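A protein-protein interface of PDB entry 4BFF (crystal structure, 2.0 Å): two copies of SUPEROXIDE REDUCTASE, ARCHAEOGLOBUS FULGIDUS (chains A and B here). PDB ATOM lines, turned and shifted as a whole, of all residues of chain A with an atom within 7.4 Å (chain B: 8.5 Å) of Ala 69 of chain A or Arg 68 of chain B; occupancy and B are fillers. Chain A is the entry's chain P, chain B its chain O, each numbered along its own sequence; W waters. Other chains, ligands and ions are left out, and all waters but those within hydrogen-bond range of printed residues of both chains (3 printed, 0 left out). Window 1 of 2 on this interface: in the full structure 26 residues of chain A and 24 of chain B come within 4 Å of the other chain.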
ATOM      1  N   ILE A  48     -34.049  20.474  13.469  1.00  0.00           N
ATOM      2  CA  ILE A  48     -32.875  19.672  13.175  1.00  0.00           C
ATOM      3  C   ILE A  48     -31.699  20.635  13.130  1.00  0.00           C
ATOM      4  O   ILE A  48     -31.786  21.671  12.478  1.00  0.00           O
ATOM      5  CB  ILE A  48     -33.025  18.943  11.818  1.00  0.00           C
ATOM      6  CG1 ILE A  48     -34.357  18.196  11.778  1.00  0.00           C
ATOM      7  CG2 ILE A  48     -31.854  17.985  11.575  1.00  0.00           C
ATOM      8  CD1 ILE A  48     -34.456  17.103  12.802  1.00  0.00           C
ATOM      9  N   ALA A  49     -30.616  20.325  13.839  1.00  0.00           N
ATOM     10  CA  ALA A  49     -29.482  21.241  13.878  1.00  0.00           C
ATOM     11  C   ALA A  49     -28.390  20.933  12.850  1.00  0.00           C
ATOM     12  O   ALA A  49     -27.728  21.853  12.364  1.00  0.00           O
ATOM     13  CB  ALA A  49     -28.879  21.323  15.283  1.00  0.00           C
ATOM     14  N   TRP A  50     -28.196  19.658  12.515  1.00  0.00           N
ATOM     15  CA  TRP A  50     -27.103  19.301  11.605  1.00  0.00           C
ATOM     16  C   TRP A  50     -27.127  17.908  11.001  1.00  0.00           C
ATOM     17  O   TRP A  50     -27.713  16.976  11.541  1.00  0.00           O
ATOM     18  CB  TRP A  50     -25.730  19.530  12.260  1.00  0.00           C
ATOM     19  CG  TRP A  50     -25.495  18.876  13.593  1.00  0.00           C
ATOM     20  CD1 TRP A  50     -25.477  19.504  14.817  1.00  0.00           C
ATOM     21  CD2 TRP A  50     -25.207  17.488  13.853  1.00  0.00           C
ATOM     22  NE1 TRP A  50     -25.200  18.597  15.809  1.00  0.00           N
ATOM     23  CE2 TRP A  50     -25.023  17.356  15.251  1.00  0.00           C
ATOM     24  CE3 TRP A  50     -25.069  16.349  13.043  1.00  0.00           C
ATOM     25  CZ2 TRP A  50     -24.728  16.132  15.861  1.00  0.00           C
ATOM     26  CZ3 TRP A  50     -24.775  15.120  13.656  1.00  0.00           C
ATOM     27  CH2 TRP A  50     -24.608  15.031  15.053  1.00  0.00           C
ATOM     28  N   ILE A  51     -26.447  17.785   9.865  1.00  0.00           N
ATOM     29  CA  ILE A  51     -26.272  16.509   9.199  1.00  0.00           C
ATOM     30  C   ILE A  51     -24.780  16.349   8.919  1.00  0.00           C
ATOM     31  O   ILE A  51     -24.136  17.290   8.462  1.00  0.00           O
ATOM     32  CB  ILE A  51     -27.046  16.460   7.852  1.00  0.00           C
ATOM     33  CG1 ILE A  51     -28.555  16.365   8.086  1.00  0.00           C
ATOM     34  CG2 ILE A  51     -26.569  15.286   6.979  1.00  0.00           C
ATOM     35  CD1 ILE A  51     -29.372  16.494   6.805  1.00  0.00           C
ATOM     36  N   GLU A  52     -24.246  15.160   9.182  1.00  0.00           N
ATOM     37  CA  GLU A  52     -22.839  14.860   8.924  1.00  0.00           C
ATOM     38  C   GLU A  52     -22.711  13.586   8.089  1.00  0.00           C
ATOM     39  O   GLU A  52     -23.313  12.563   8.423  1.00  0.00           O
ATOM     40  CB  GLU A  52     -22.111  14.687  10.246  1.00  0.00           C
ATOM     41  CG  GLU A  52     -20.626  14.438  10.133  1.00  0.00           C
ATOM     42  CD  GLU A  52     -19.883  14.900  11.371  1.00  0.00           C
ATOM     43  OE1 GLU A  52     -20.324  14.568  12.497  1.00  0.00           O
ATOM     44  OE2 GLU A  52     -18.868  15.611  11.208  1.00  0.00           O
ATOM     45  N   LEU A  53     -21.928  13.642   7.006  1.00  0.00           N
ATOM     46  CA  LEU A  53     -21.839  12.505   6.087  1.00  0.00           C
ATOM     47  C   LEU A  53     -20.497  11.793   6.204  1.00  0.00           C
ATOM     48  O   LEU A  53     -19.454  12.430   6.210  1.00  0.00           O
ATOM     49  CB  LEU A  53     -22.084  12.937   4.634  1.00  0.00           C
ATOM     50  CG  LEU A  53     -21.990  11.813   3.589  1.00  0.00           C
ATOM     51  CD1 LEU A  53     -23.100  10.770   3.797  1.00  0.00           C
ATOM     52  CD2 LEU A  53     -22.018  12.345   2.145  1.00  0.00           C
ATOM     53  N   GLY A  67     -18.186  15.523   5.140  1.00  0.00           N
ATOM     54  CA  GLY A  67     -18.554  16.887   5.449  1.00  0.00           C
ATOM     55  C   GLY A  67     -19.594  16.978   6.561  1.00  0.00           C
ATOM     56  O   GLY A  67     -20.133  15.973   7.039  1.00  0.00           O
ATOM     57  N   ARG A  68     -19.862  18.203   6.969  1.00  0.00           N
ATOM     58  CA  ARG A  68     -20.859  18.483   7.991  1.00  0.00           C
ATOM     59  C   ARG A  68     -21.616  19.735   7.582  1.00  0.00           C
ATOM     60  O   ARG A  68     -21.020  20.713   7.125  1.00  0.00           O
ATOM     61  CB  ARG A  68     -20.183  18.678   9.346  1.00  0.00           C
ATOM     62  CG  ARG A  68     -21.132  19.164  10.486  1.00  0.00           C
ATOM     63  CD  ARG A  68     -20.351  19.276  11.782  1.00  0.00           C
ATOM     64  NE  ARG A  68     -21.077  19.918  12.877  1.00  0.00           N
ATOM     65  CZ  ARG A  68     -21.738  19.256  13.821  1.00  0.00           C
ATOM     66  NH1 ARG A  68     -21.789  17.921  13.794  1.00  0.00           N
ATOM     67  NH2 ARG A  68     -22.351  19.925  14.790  1.00  0.00           N
ATOM     68  N   ALA A  69     -22.935  19.691   7.715  1.00  0.00           N
ATOM     69  CA  ALA A  69     -23.765  20.844   7.393  1.00  0.00           C
ATOM     70  C   ALA A  69     -24.579  21.242   8.619  1.00  0.00           C
ATOM     71  O   ALA A  69     -25.328  20.433   9.170  1.00  0.00           O
ATOM     72  CB  ALA A  69     -24.673  20.543   6.216  1.00  0.00           C
ATOM     73  N   GLU A  70     -24.396  22.479   9.063  1.00  0.00           N
ATOM     74  CA  GLU A  70     -25.201  23.019  10.151  1.00  0.00           C
ATOM     75  C   GLU A  70     -26.283  23.895   9.585  1.00  0.00           C
ATOM     76  O   GLU A  70     -26.047  24.672   8.661  1.00  0.00           O
ATOM     77  CB  GLU A  70     -24.355  23.861  11.098  1.00  0.00           C
ATOM     78  CG  GLU A  70     -23.284  23.086  11.831  1.00  0.00           C
ATOM     79  CD  GLU A  70     -22.112  23.962  12.193  1.00  0.00           C
ATOM     80  OE1 GLU A  70     -22.220  25.191  12.006  1.00  0.00           O
ATOM     81  OE2 GLU A  70     -21.085  23.427  12.651  1.00  0.00           O
ATOM     82  N   PHE A  71     -27.475  23.776  10.159  1.00  0.00           N
ATOM     83  CA  PHE A  71     -28.599  24.603   9.795  1.00  0.00           C
ATOM     84  C   PHE A  71     -28.885  25.518  10.985  1.00  0.00           C
ATOM     85  O   PHE A  71     -29.329  25.064  12.033  1.00  0.00           O
ATOM     86  CB  PHE A  71     -29.765  23.687   9.459  1.00  0.00           C
ATOM     87  CG  PHE A  71     -29.347  22.484   8.667  1.00  0.00           C
ATOM     88  CD1 PHE A  71     -28.796  22.639   7.412  1.00  0.00           C
ATOM     89  CD2 PHE A  71     -29.478  21.207   9.190  1.00  0.00           C
ATOM     90  CE1 PHE A  71     -28.395  21.534   6.659  1.00  0.00           C
ATOM     91  CE2 PHE A  71     -29.069  20.099   8.471  1.00  0.00           C
ATOM     92  CZ  PHE A  71     -28.530  20.265   7.189  1.00  0.00           C
ATOM     93  N   ALA A  72     -28.607  26.806  10.806  1.00  0.00           N
ATOM     94  CA  ALA A  72     -28.424  27.731  11.920  1.00  0.00           C
ATOM     95  C   ALA A  72     -29.578  28.703  12.175  1.00  0.00           C
ATOM     96  O   ALA A  72     -29.656  29.297  13.255  1.00  0.00           O
ATOM     97  CB  ALA A  72     -27.138  28.510  11.737  1.00  0.00           C
ATOM     98  N   THR A  88     -33.641  27.585   8.192  1.00  0.00           N
ATOM     99  CA  THR A  88     -32.791  26.735   7.358  1.00  0.00           C
ATOM    100  C   THR A  88     -33.323  25.302   7.256  1.00  0.00           C
ATOM    101  O   THR A  88     -33.490  24.611   8.272  1.00  0.00           O
ATOM    102  CB  THR A  88     -31.341  26.693   7.879  1.00  0.00           C
ATOM    103  OG1 THR A  88     -30.894  28.021   8.191  1.00  0.00           O
ATOM    104  CG2 THR A  88     -30.389  26.049   6.828  1.00  0.00           C
ATOM    105  N   PRO A  90     -33.316  21.377   6.735  1.00  0.00           N
ATOM    106  CA  PRO A  90     -32.300  20.346   7.000  1.00  0.00           C
ATOM    107  C   PRO A  90     -32.010  19.463   5.773  1.00  0.00           C
ATOM    108  O   PRO A  90     -32.244  18.254   5.783  1.00  0.00           O
ATOM    109  CB  PRO A  90     -32.914  19.529   8.137  1.00  0.00           C
ATOM    110  CG  PRO A  90     -34.392  19.727   8.009  1.00  0.00           C
ATOM    111  CD  PRO A  90     -34.595  21.098   7.414  1.00  0.00           C
ATOM    112  N   VAL A  91     -31.501  20.091   4.722  1.00  0.00           N
ATOM    113  CA  VAL A  91     -31.081  19.376   3.522  1.00  0.00           C
ATOM    114  C   VAL A  91     -29.717  19.884   3.082  1.00  0.00           C
ATOM    115  O   VAL A  91     -29.474  21.084   3.015  1.00  0.00           O
ATOM    116  CB  VAL A  91     -32.100  19.520   2.373  1.00  0.00           C
ATOM    117  CG1 VAL A  91     -32.527  20.966   2.218  1.00  0.00           C
ATOM    118  CG2 VAL A  91     -31.529  18.958   1.063  1.00  0.00           C
ATOM    119  N   ALA A  92     -28.823  18.949   2.789  1.00  0.00           N
ATOM    120  CA  ALA A  92     -27.463  19.288   2.403  1.00  0.00           C
ATOM    121  C   ALA A  92     -27.063  18.487   1.172  1.00  0.00           C
ATOM    122  O   ALA A  92     -27.533  17.369   0.979  1.00  0.00           O
ATOM    123  CB  ALA A  92     -26.514  18.983   3.544  1.00  0.00           C
ATOM    124  N   VAL A  93     -26.183  19.055   0.355  1.00  0.00           N
ATOM    125  CA  VAL A  93     -25.588  18.313  -0.758  1.00  0.00           C
ATOM    126  C   VAL A  93     -24.069  18.276  -0.619  1.00  0.00           C
ATOM    127  O   VAL A  93     -23.415  19.318  -0.558  1.00  0.00           O
ATOM    128  CB  VAL A  93     -25.974  18.910  -2.115  1.00  0.00           C
ATOM    129  CG1 VAL A  93     -25.314  18.117  -3.264  1.00  0.00           C
ATOM    130  CG2 VAL A  93     -27.482  18.928  -2.261  1.00  0.00           C
ATOM    131  N   PHE A  94     -23.521  17.065  -0.551  1.00  0.00           N
ATOM    132  CA  PHE A  94     -22.095  16.868  -0.362  1.00  0.00           C
ATOM    133  C   PHE A  94     -21.527  16.441  -1.707  1.00  0.00           C
ATOM    134  O   PHE A  94     -21.976  15.457  -2.289  1.00  0.00           O
ATOM    135  CB  PHE A  94     -21.839  15.782   0.692  1.00  0.00           C
ATOM    136  CG  PHE A  94     -22.476  16.062   2.047  1.00  0.00           C
ATOM    137  CD1 PHE A  94     -23.786  15.679   2.308  1.00  0.00           C
ATOM    138  CD2 PHE A  94     -21.757  16.694   3.051  1.00  0.00           C
ATOM    139  CE1 PHE A  94     -24.382  15.935   3.557  1.00  0.00           C
ATOM    140  CE2 PHE A  94     -22.334  16.954   4.291  1.00  0.00           C
ATOM    141  CZ  PHE A  94     -23.648  16.574   4.547  1.00  0.00           C
ATOM    142  N   PHE A 107     -25.403  10.964   9.777  1.00  0.00           N
ATOM    143  CA  PHE A 107     -25.793  11.239  11.156  1.00  0.00           C
ATOM    144  C   PHE A 107     -26.535  12.571  11.235  1.00  0.00           C
ATOM    145  O   PHE A 107     -26.183  13.523  10.535  1.00  0.00           O
ATOM    146  CB  PHE A 107     -24.553  11.317  12.063  1.00  0.00           C
ATOM    147  CG  PHE A 107     -23.829  10.022  12.198  1.00  0.00           C
ATOM    148  CD1 PHE A 107     -24.445   8.933  12.782  1.00  0.00           C
ATOM    149  CD2 PHE A 107     -22.524   9.888  11.743  1.00  0.00           C
ATOM    150  CE1 PHE A 107     -23.775   7.723  12.910  1.00  0.00           C
ATOM    151  CE2 PHE A 107     -21.854   8.689  11.864  1.00  0.00           C
ATOM    152  CZ  PHE A 107     -22.482   7.602  12.447  1.00  0.00           C
ATOM    153  N   ALA B  49     -11.415  24.669   3.724  1.00  0.00           N
ATOM    154  CA  ALA B  49     -11.952  23.892   4.849  1.00  0.00           C
ATOM    155  C   ALA B  49     -13.451  24.096   5.101  1.00  0.00           C
ATOM    156  O   ALA B  49     -14.153  23.158   5.482  1.00  0.00           O
ATOM    157  CB  ALA B  49     -11.148  24.152   6.124  1.00  0.00           C
ATOM    158  N   TRP B  50     -13.948  25.312   4.905  1.00  0.00           N
ATOM    159  CA  TRP B  50     -15.381  25.533   5.095  1.00  0.00           C
ATOM    160  C   TRP B  50     -15.941  26.717   4.340  1.00  0.00           C
ATOM    161  O   TRP B  50     -15.187  27.566   3.878  1.00  0.00           O
ATOM    162  CB  TRP B  50     -15.734  25.676   6.591  1.00  0.00           C
ATOM    163  CG  TRP B  50     -14.857  26.591   7.389  1.00  0.00           C
ATOM    164  CD1 TRP B  50     -13.810  26.228   8.189  1.00  0.00           C
ATOM    165  CD2 TRP B  50     -14.974  28.013   7.504  1.00  0.00           C
ATOM    166  NE1 TRP B  50     -13.254  27.338   8.776  1.00  0.00           N
ATOM    167  CE2 TRP B  50     -13.961  28.449   8.380  1.00  0.00           C
ATOM    168  CE3 TRP B  50     -15.831  28.965   6.941  1.00  0.00           C
ATOM    169  CZ2 TRP B  50     -13.777  29.789   8.707  1.00  0.00           C
ATOM    170  CZ3 TRP B  50     -15.650  30.290   7.261  1.00  0.00           C
ATOM    171  CH2 TRP B  50     -14.631  30.695   8.140  1.00  0.00           C
ATOM    172  N   ILE B  51     -17.275  26.752   4.245  1.00  0.00           N
ATOM    173  CA  ILE B  51     -18.017  27.897   3.740  1.00  0.00           C
ATOM    174  C   ILE B  51     -19.188  28.187   4.686  1.00  0.00           C
ATOM    175  O   ILE B  51     -19.898  27.278   5.116  1.00  0.00           O
ATOM    176  CB  ILE B  51     -18.571  27.623   2.329  1.00  0.00           C
ATOM    177  CG1 ILE B  51     -17.459  27.730   1.269  1.00  0.00           C
ATOM    178  CG2 ILE B  51     -19.693  28.558   1.996  1.00  0.00           C
ATOM    179  CD1 ILE B  51     -17.944  27.365  -0.124  1.00  0.00           C
ATOM    180  N   GLU B  52     -19.389  29.455   5.012  1.00  0.00           N
ATOM    181  CA  GLU B  52     -20.457  29.833   5.933  1.00  0.00           C
ATOM    182  C   GLU B  52     -21.279  30.919   5.281  1.00  0.00           C
ATOM    183  O   GLU B  52     -20.723  31.861   4.716  1.00  0.00           O
ATOM    184  CB  GLU B  52     -19.870  30.339   7.246  1.00  0.00           C
ATOM    185  CG  GLU B  52     -20.904  30.582   8.317  1.00  0.00           C
ATOM    186  CD  GLU B  52     -20.270  30.869   9.650  1.00  0.00           C
ATOM    187  OE1 GLU B  52     -19.291  31.648   9.680  1.00  0.00           O
ATOM    188  OE2 GLU B  52     -20.741  30.308  10.663  1.00  0.00           O
ATOM    189  N   LEU B  53     -22.598  30.769   5.326  1.00  0.00           N
ATOM    190  CA  LEU B  53     -23.501  31.716   4.668  1.00  0.00           C
ATOM    191  C   LEU B  53     -24.341  32.517   5.658  1.00  0.00           C
ATOM    192  O   LEU B  53     -25.024  31.946   6.511  1.00  0.00           O
ATOM    193  CB  LEU B  53     -24.427  30.990   3.688  1.00  0.00           C
ATOM    194  CG  LEU B  53     -25.481  31.878   3.025  1.00  0.00           C
ATOM    195  CD1 LEU B  53     -24.844  32.782   1.971  1.00  0.00           C
ATOM    196  CD2 LEU B  53     -26.608  31.042   2.437  1.00  0.00           C
ATOM    197  N   VAL B  54     -24.317  33.835   5.491  1.00  0.00           N
ATOM    198  CA  VAL B  54     -25.068  34.767   6.328  1.00  0.00           C
ATOM    199  C   VAL B  54     -26.106  35.533   5.507  1.00  0.00           C
ATOM    200  O   VAL B  54     -25.823  35.968   4.390  1.00  0.00           O
ATOM    201  CB  VAL B  54     -24.104  35.758   6.999  1.00  0.00           C
ATOM    202  CG1 VAL B  54     -24.851  36.893   7.650  1.00  0.00           C
ATOM    203  CG2 VAL B  54     -23.244  35.028   8.016  1.00  0.00           C
ATOM    204  N   VAL B  65     -26.875  33.836  10.598  1.00  0.00           N
ATOM    205  CA  VAL B  65     -26.136  32.791   9.918  1.00  0.00           C
ATOM    206  C   VAL B  65     -27.211  31.846   9.411  1.00  0.00           C
ATOM    207  O   VAL B  65     -28.114  31.465  10.160  1.00  0.00           O
ATOM    208  CB  VAL B  65     -25.163  32.046  10.874  1.00  0.00           C
ATOM    209  CG1 VAL B  65     -24.467  30.905  10.146  1.00  0.00           C
ATOM    210  CG2 VAL B  65     -24.143  33.021  11.468  1.00  0.00           C
ATOM    211  N   VAL B  66     -27.160  31.521   8.130  1.00  0.00           N
ATOM    212  CA  VAL B  66     -28.088  30.549   7.574  1.00  0.00           C
ATOM    213  C   VAL B  66     -27.542  29.144   7.840  1.00  0.00           C
ATOM    214  O   VAL B  66     -28.274  28.221   8.184  1.00  0.00           O
ATOM    215  CB  VAL B  66     -28.235  30.733   6.050  1.00  0.00           C
ATOM    216  CG1 VAL B  66     -29.008  29.571   5.443  1.00  0.00           C
ATOM    217  CG2 VAL B  66     -28.885  32.081   5.707  1.00  0.00           C
ATOM    218  N   GLY B  67     -26.238  28.986   7.674  1.00  0.00           N
ATOM    219  CA  GLY B  67     -25.643  27.666   7.788  1.00  0.00           C
ATOM    220  C   GLY B  67     -24.151  27.651   7.564  1.00  0.00           C
ATOM    221  O   GLY B  67     -23.547  28.675   7.253  1.00  0.00           O
ATOM    222  N   ARG B  68     -23.554  26.476   7.741  1.00  0.00           N
ATOM    223  CA  ARG B  68     -22.120  26.321   7.587  1.00  0.00           C
ATOM    224  C   ARG B  68     -21.839  24.930   7.069  1.00  0.00           C
ATOM    225  O   ARG B  68     -22.443  23.962   7.528  1.00  0.00           O
ATOM    226  CB  ARG B  68     -21.391  26.555   8.910  1.00  0.00           C
ATOM    227  CG  ARG B  68     -19.876  26.376   8.816  1.00  0.00           C
ATOM    228  CD  ARG B  68     -19.205  27.051  10.012  1.00  0.00           C
ATOM    229  NE  ARG B  68     -17.785  26.739  10.148  1.00  0.00           N
ATOM    230  CZ  ARG B  68     -17.329  25.664  10.772  1.00  0.00           C
ATOM    231  NH1 ARG B  68     -18.188  24.802  11.303  1.00  0.00           N
ATOM    232  NH2 ARG B  68     -16.023  25.454  10.864  1.00  0.00           N
ATOM    233  N   ALA B  69     -20.939  24.852   6.092  1.00  0.00           N
ATOM    234  CA  ALA B  69     -20.583  23.601   5.451  1.00  0.00           C
ATOM    235  C   ALA B  69     -19.091  23.307   5.654  1.00  0.00           C
ATOM    236  O   ALA B  69     -18.226  24.117   5.327  1.00  0.00           O
ATOM    237  CB  ALA B  69     -20.933  23.649   3.941  1.00  0.00           C
ATOM    238  N   GLU B  70     -18.798  22.152   6.228  1.00  0.00           N
ATOM    239  CA  GLU B  70     -17.423  21.753   6.390  1.00  0.00           C
ATOM    240  C   GLU B  70     -17.045  20.742   5.318  1.00  0.00           C
ATOM    241  O   GLU B  70     -17.824  19.846   5.010  1.00  0.00           O
ATOM    242  CB  GLU B  70     -17.211  21.195   7.796  1.00  0.00           C
ATOM    243  CG  GLU B  70     -17.387  22.250   8.872  1.00  0.00           C
ATOM    244  CD  GLU B  70     -17.408  21.668  10.269  1.00  0.00           C
ATOM    245  OE1 GLU B  70     -16.855  20.575  10.487  1.00  0.00           O
ATOM    246  OE2 GLU B  70     -17.988  22.303  11.159  1.00  0.00           O
ATOM    247  N   PHE B  71     -15.867  20.918   4.725  1.00  0.00           N
ATOM    248  CA  PHE B  71     -15.315  19.954   3.754  1.00  0.00           C
ATOM    249  C   PHE B  71     -14.122  19.242   4.375  1.00  0.00           C
ATOM    250  O   PHE B  71     -13.052  19.822   4.504  1.00  0.00           O
ATOM    251  CB  PHE B  71     -14.928  20.690   2.470  1.00  0.00           C
ATOM    252  CG  PHE B  71     -15.941  21.713   2.072  1.00  0.00           C
ATOM    253  CD1 PHE B  71     -17.221  21.313   1.704  1.00  0.00           C
ATOM    254  CD2 PHE B  71     -15.647  23.068   2.135  1.00  0.00           C
ATOM    255  CE1 PHE B  71     -18.180  22.245   1.370  1.00  0.00           C
ATOM    256  CE2 PHE B  71     -16.601  24.009   1.800  1.00  0.00           C
ATOM    257  CZ  PHE B  71     -17.865  23.597   1.411  1.00  0.00           C
ATOM    258  N   ALA B  92     -21.277  24.181  -1.543  1.00  0.00           N
ATOM    259  CA  ALA B  92     -22.347  23.898  -0.610  1.00  0.00           C
ATOM    260  C   ALA B  92     -23.662  24.458  -1.140  1.00  0.00           C
ATOM    261  O   ALA B  92     -23.694  25.512  -1.776  1.00  0.00           O
ATOM    262  CB  ALA B  92     -22.025  24.512   0.735  1.00  0.00           C
ATOM    263  N   VAL B  93     -24.752  23.755  -0.868  1.00  0.00           N
ATOM    264  CA  VAL B  93     -26.074  24.271  -1.202  1.00  0.00           C
ATOM    265  C   VAL B  93     -26.889  24.530   0.074  1.00  0.00           C
ATOM    266  O   VAL B  93     -27.085  23.631   0.904  1.00  0.00           O
ATOM    267  CB  VAL B  93     -26.815  23.337  -2.176  1.00  0.00           C
ATOM    268  CG1 VAL B  93     -28.225  23.803  -2.387  1.00  0.00           C
ATOM    269  CG2 VAL B  93     -26.078  23.271  -3.506  1.00  0.00           C
ATOM    270  N   PHE B  94     -27.325  25.778   0.238  1.00  0.00           N
ATOM    271  CA  PHE B  94     -28.118  26.176   1.406  1.00  0.00           C
ATOM    272  C   PHE B  94     -29.569  26.400   1.003  1.00  0.00           C
ATOM    273  O   PHE B  94     -29.844  27.255   0.169  1.00  0.00           O
ATOM    274  CB  PHE B  94     -27.564  27.465   2.009  1.00  0.00           C
ATOM    275  CG  PHE B  94     -26.155  27.347   2.502  1.00  0.00           C
ATOM    276  CD1 PHE B  94     -25.890  26.919   3.801  1.00  0.00           C
ATOM    277  CD2 PHE B  94     -25.088  27.647   1.665  1.00  0.00           C
ATOM    278  CE1 PHE B  94     -24.584  26.797   4.263  1.00  0.00           C
ATOM    279  CE2 PHE B  94     -23.780  27.534   2.118  1.00  0.00           C
ATOM    280  CZ  PHE B  94     -23.526  27.107   3.428  1.00  0.00           C
ATOM    281  N   PHE B 107     -18.572  33.506   3.874  1.00  0.00           N
ATOM    282  CA  PHE B 107     -17.206  33.492   4.386  1.00  0.00           C
ATOM    283  C   PHE B 107     -16.565  32.141   4.077  1.00  0.00           C
ATOM    284  O   PHE B 107     -17.223  31.101   4.185  1.00  0.00           O
ATOM    285  CB  PHE B 107     -17.177  33.775   5.889  1.00  0.00           C
ATOM    286  CG  PHE B 107     -17.723  35.140   6.262  1.00  0.00           C
ATOM    287  CD1 PHE B 107     -16.983  36.286   6.029  1.00  0.00           C
ATOM    288  CD2 PHE B 107     -18.982  35.272   6.834  1.00  0.00           C
ATOM    289  CE1 PHE B 107     -17.481  37.540   6.376  1.00  0.00           C
ATOM    290  CE2 PHE B 107     -19.483  36.526   7.180  1.00  0.00           C
ATOM    291  CZ  PHE B 107     -18.736  37.657   6.943  1.00  0.00           C
ATOM    292  N   TYR B 109     -12.590  29.729   4.141  1.00  0.00           N
ATOM    293  CA  TYR B 109     -11.260  29.610   4.749  1.00  0.00           C
ATOM    294  C   TYR B 109     -10.341  28.604   4.015  1.00  0.00           C
ATOM    295  O   TYR B 109     -10.729  27.463   3.775  1.00  0.00           O
ATOM    296  CB  TYR B 109     -11.402  29.224   6.218  1.00  0.00           C
ATOM    297  CG  TYR B 109     -10.082  28.987   6.931  1.00  0.00           C
ATOM    298  CD1 TYR B 109      -9.160  30.014   7.064  1.00  0.00           C
ATOM    299  CD2 TYR B 109      -9.765  27.736   7.477  1.00  0.00           C
ATOM    300  CE1 TYR B 109      -7.950  29.819   7.706  1.00  0.00           C
ATOM    301  CE2 TYR B 109      -8.559  27.536   8.147  1.00  0.00           C
ATOM    302  CZ  TYR B 109      -7.658  28.588   8.248  1.00  0.00           C
ATOM    303  OH  TYR B 109      -6.452  28.434   8.888  1.00  0.00           O
HETATM  304  O   HOH W   1     -29.575  22.253   0.005  1.00  0.00           O
HETATM  305  O   HOH W   2     -29.077  31.683  12.805  1.00  0.00           O
HETATM  306  O   HOH W   3     -24.617  21.853   1.257  1.00  0.00           O
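Among the printed residues, pairs that only touch across the chains: Gly 67 of chain A with Glu 70 of chain B, Arg 68 of chain A with Arg 68 of chain B, Arg 68 of chain A with Ala 69 of chain B, Ala 69 of chain A with Arg 68 of chain B, Glu 70 of chain A with Gly 67 of chain B, Glu 70 of chain A with Glu 70 of chain B, Phe 71 of chain A with Val 66 of chain B and Ala 72 of chain A with Val 65 of chain B.
Arg 68 of chain B touches its own counterpart, Arg 68 of chain A.
Arg 68 of chain A touches Ala 69 of chain B, and with the chains exchanged Ala 69 of chain A touches Arg 68 of chain B.
Arg 68 of chain A touches Glu 70 of chain B, and with the chains exchanged Glu 70 of chain A touches Arg 68 of chain B.
Glu 70 of chain B touches its own counterpart, Glu 70 of chain A.
Of the 12 pairs that touch across the chains among the printed residues, 8 have their exchanged pair printed and touching as well.
The backbone carbonyl oxygen of Leu 53 of chain B is in hydrogen-bond range of the backbone NH of Val 66 of chain B (2.7 Å).
The backbone NH (N) of Phe 71 of chain A lies within hydrogen-bond range of the backbone carbonyl oxygen (O) of Ala 49 of chain A (2.9 Å).
The backbone carbonyl oxygen (O) of Ile 51 of chain B sits at hydrogen-bond distance from the backbone NH (N) of Ala 69 of chain B (2.8 Å).
The backbone NH of Leu 53 of chain B is in hydrogen-bond range of the backbone carbonyl oxygen of Gly 67 of chain B.
Hydrophobic or aromatic side chains of chain A within 4 Å of the printed part of chain B: Ala 72.
The backbone carbonyl oxygen (O) of Val 66 of chain B lies within hydrogen-bond range of the side-chain hydroxyl (OG1) of Thr 88 of chain A, 2.6 Å away.
NH1 of Arg 68 of chain B is in salt-bridge range of OE2 of Glu 70 of chain A (3.5 Å).
The backbone NH (N) of Ala 72 of chain A is in hydrogen-bond range of the backbone carbonyl oxygen (O) of Val 66 of chain B.
The backbone NH of Glu 70 of chain B is in hydrogen-bond range of the backbone carbonyl oxygen of Arg 68 of chain A (2.8 Å).
Ala 69 of chain A touches one residue of chain B.
Arg 68 of chain B touches three residues of chain A.
Of chain B, only Gly 67, Arg 68 and Glu 70 come within 4 Å of Glu 70 of chain A.
Of the printed residues of chain B, Ala 72 of chain A touches Val 65 and Val 66.
Of the printed residues of chain A, Gly 67 of chain B touches Glu 70 (3.1 Å).
Of the printed residues of chain A, Val 65 of chain B touches Ala 72.
Of the printed residues of chain B, Arg 68 of chain A touches Arg 68 (3.6 Å), Ala 69 (3.4 Å) and Glu 70 (2.8 Å).
Phe 107 of chain B touches none of the printed residues of chain A.
The nearest residue of chain B that does not touch Ala 69 of chain A is Ala 69 of chain B (4.6 Å).
The nearest residue of chain A that does not touch Arg 68 of chain B is Phe 71 of chain A (5.3 Å).
Water W2 bridges the backbone carbonyl oxygen (O) of Ala 72 of chain A and the backbone carbonyl oxygen (O) of Val 65 of chain B.
Water W3 bridges N of Val 93 of chain B and N of Val 93 of chain A.
Water W1 lies within hydrogen-bond range of the backbone carbonyl oxygen (O) of Val 93 of chain B (3.0 Å) and the backbone carbonyl oxygen (O) of Val 91 of chain A (3.2 Å).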
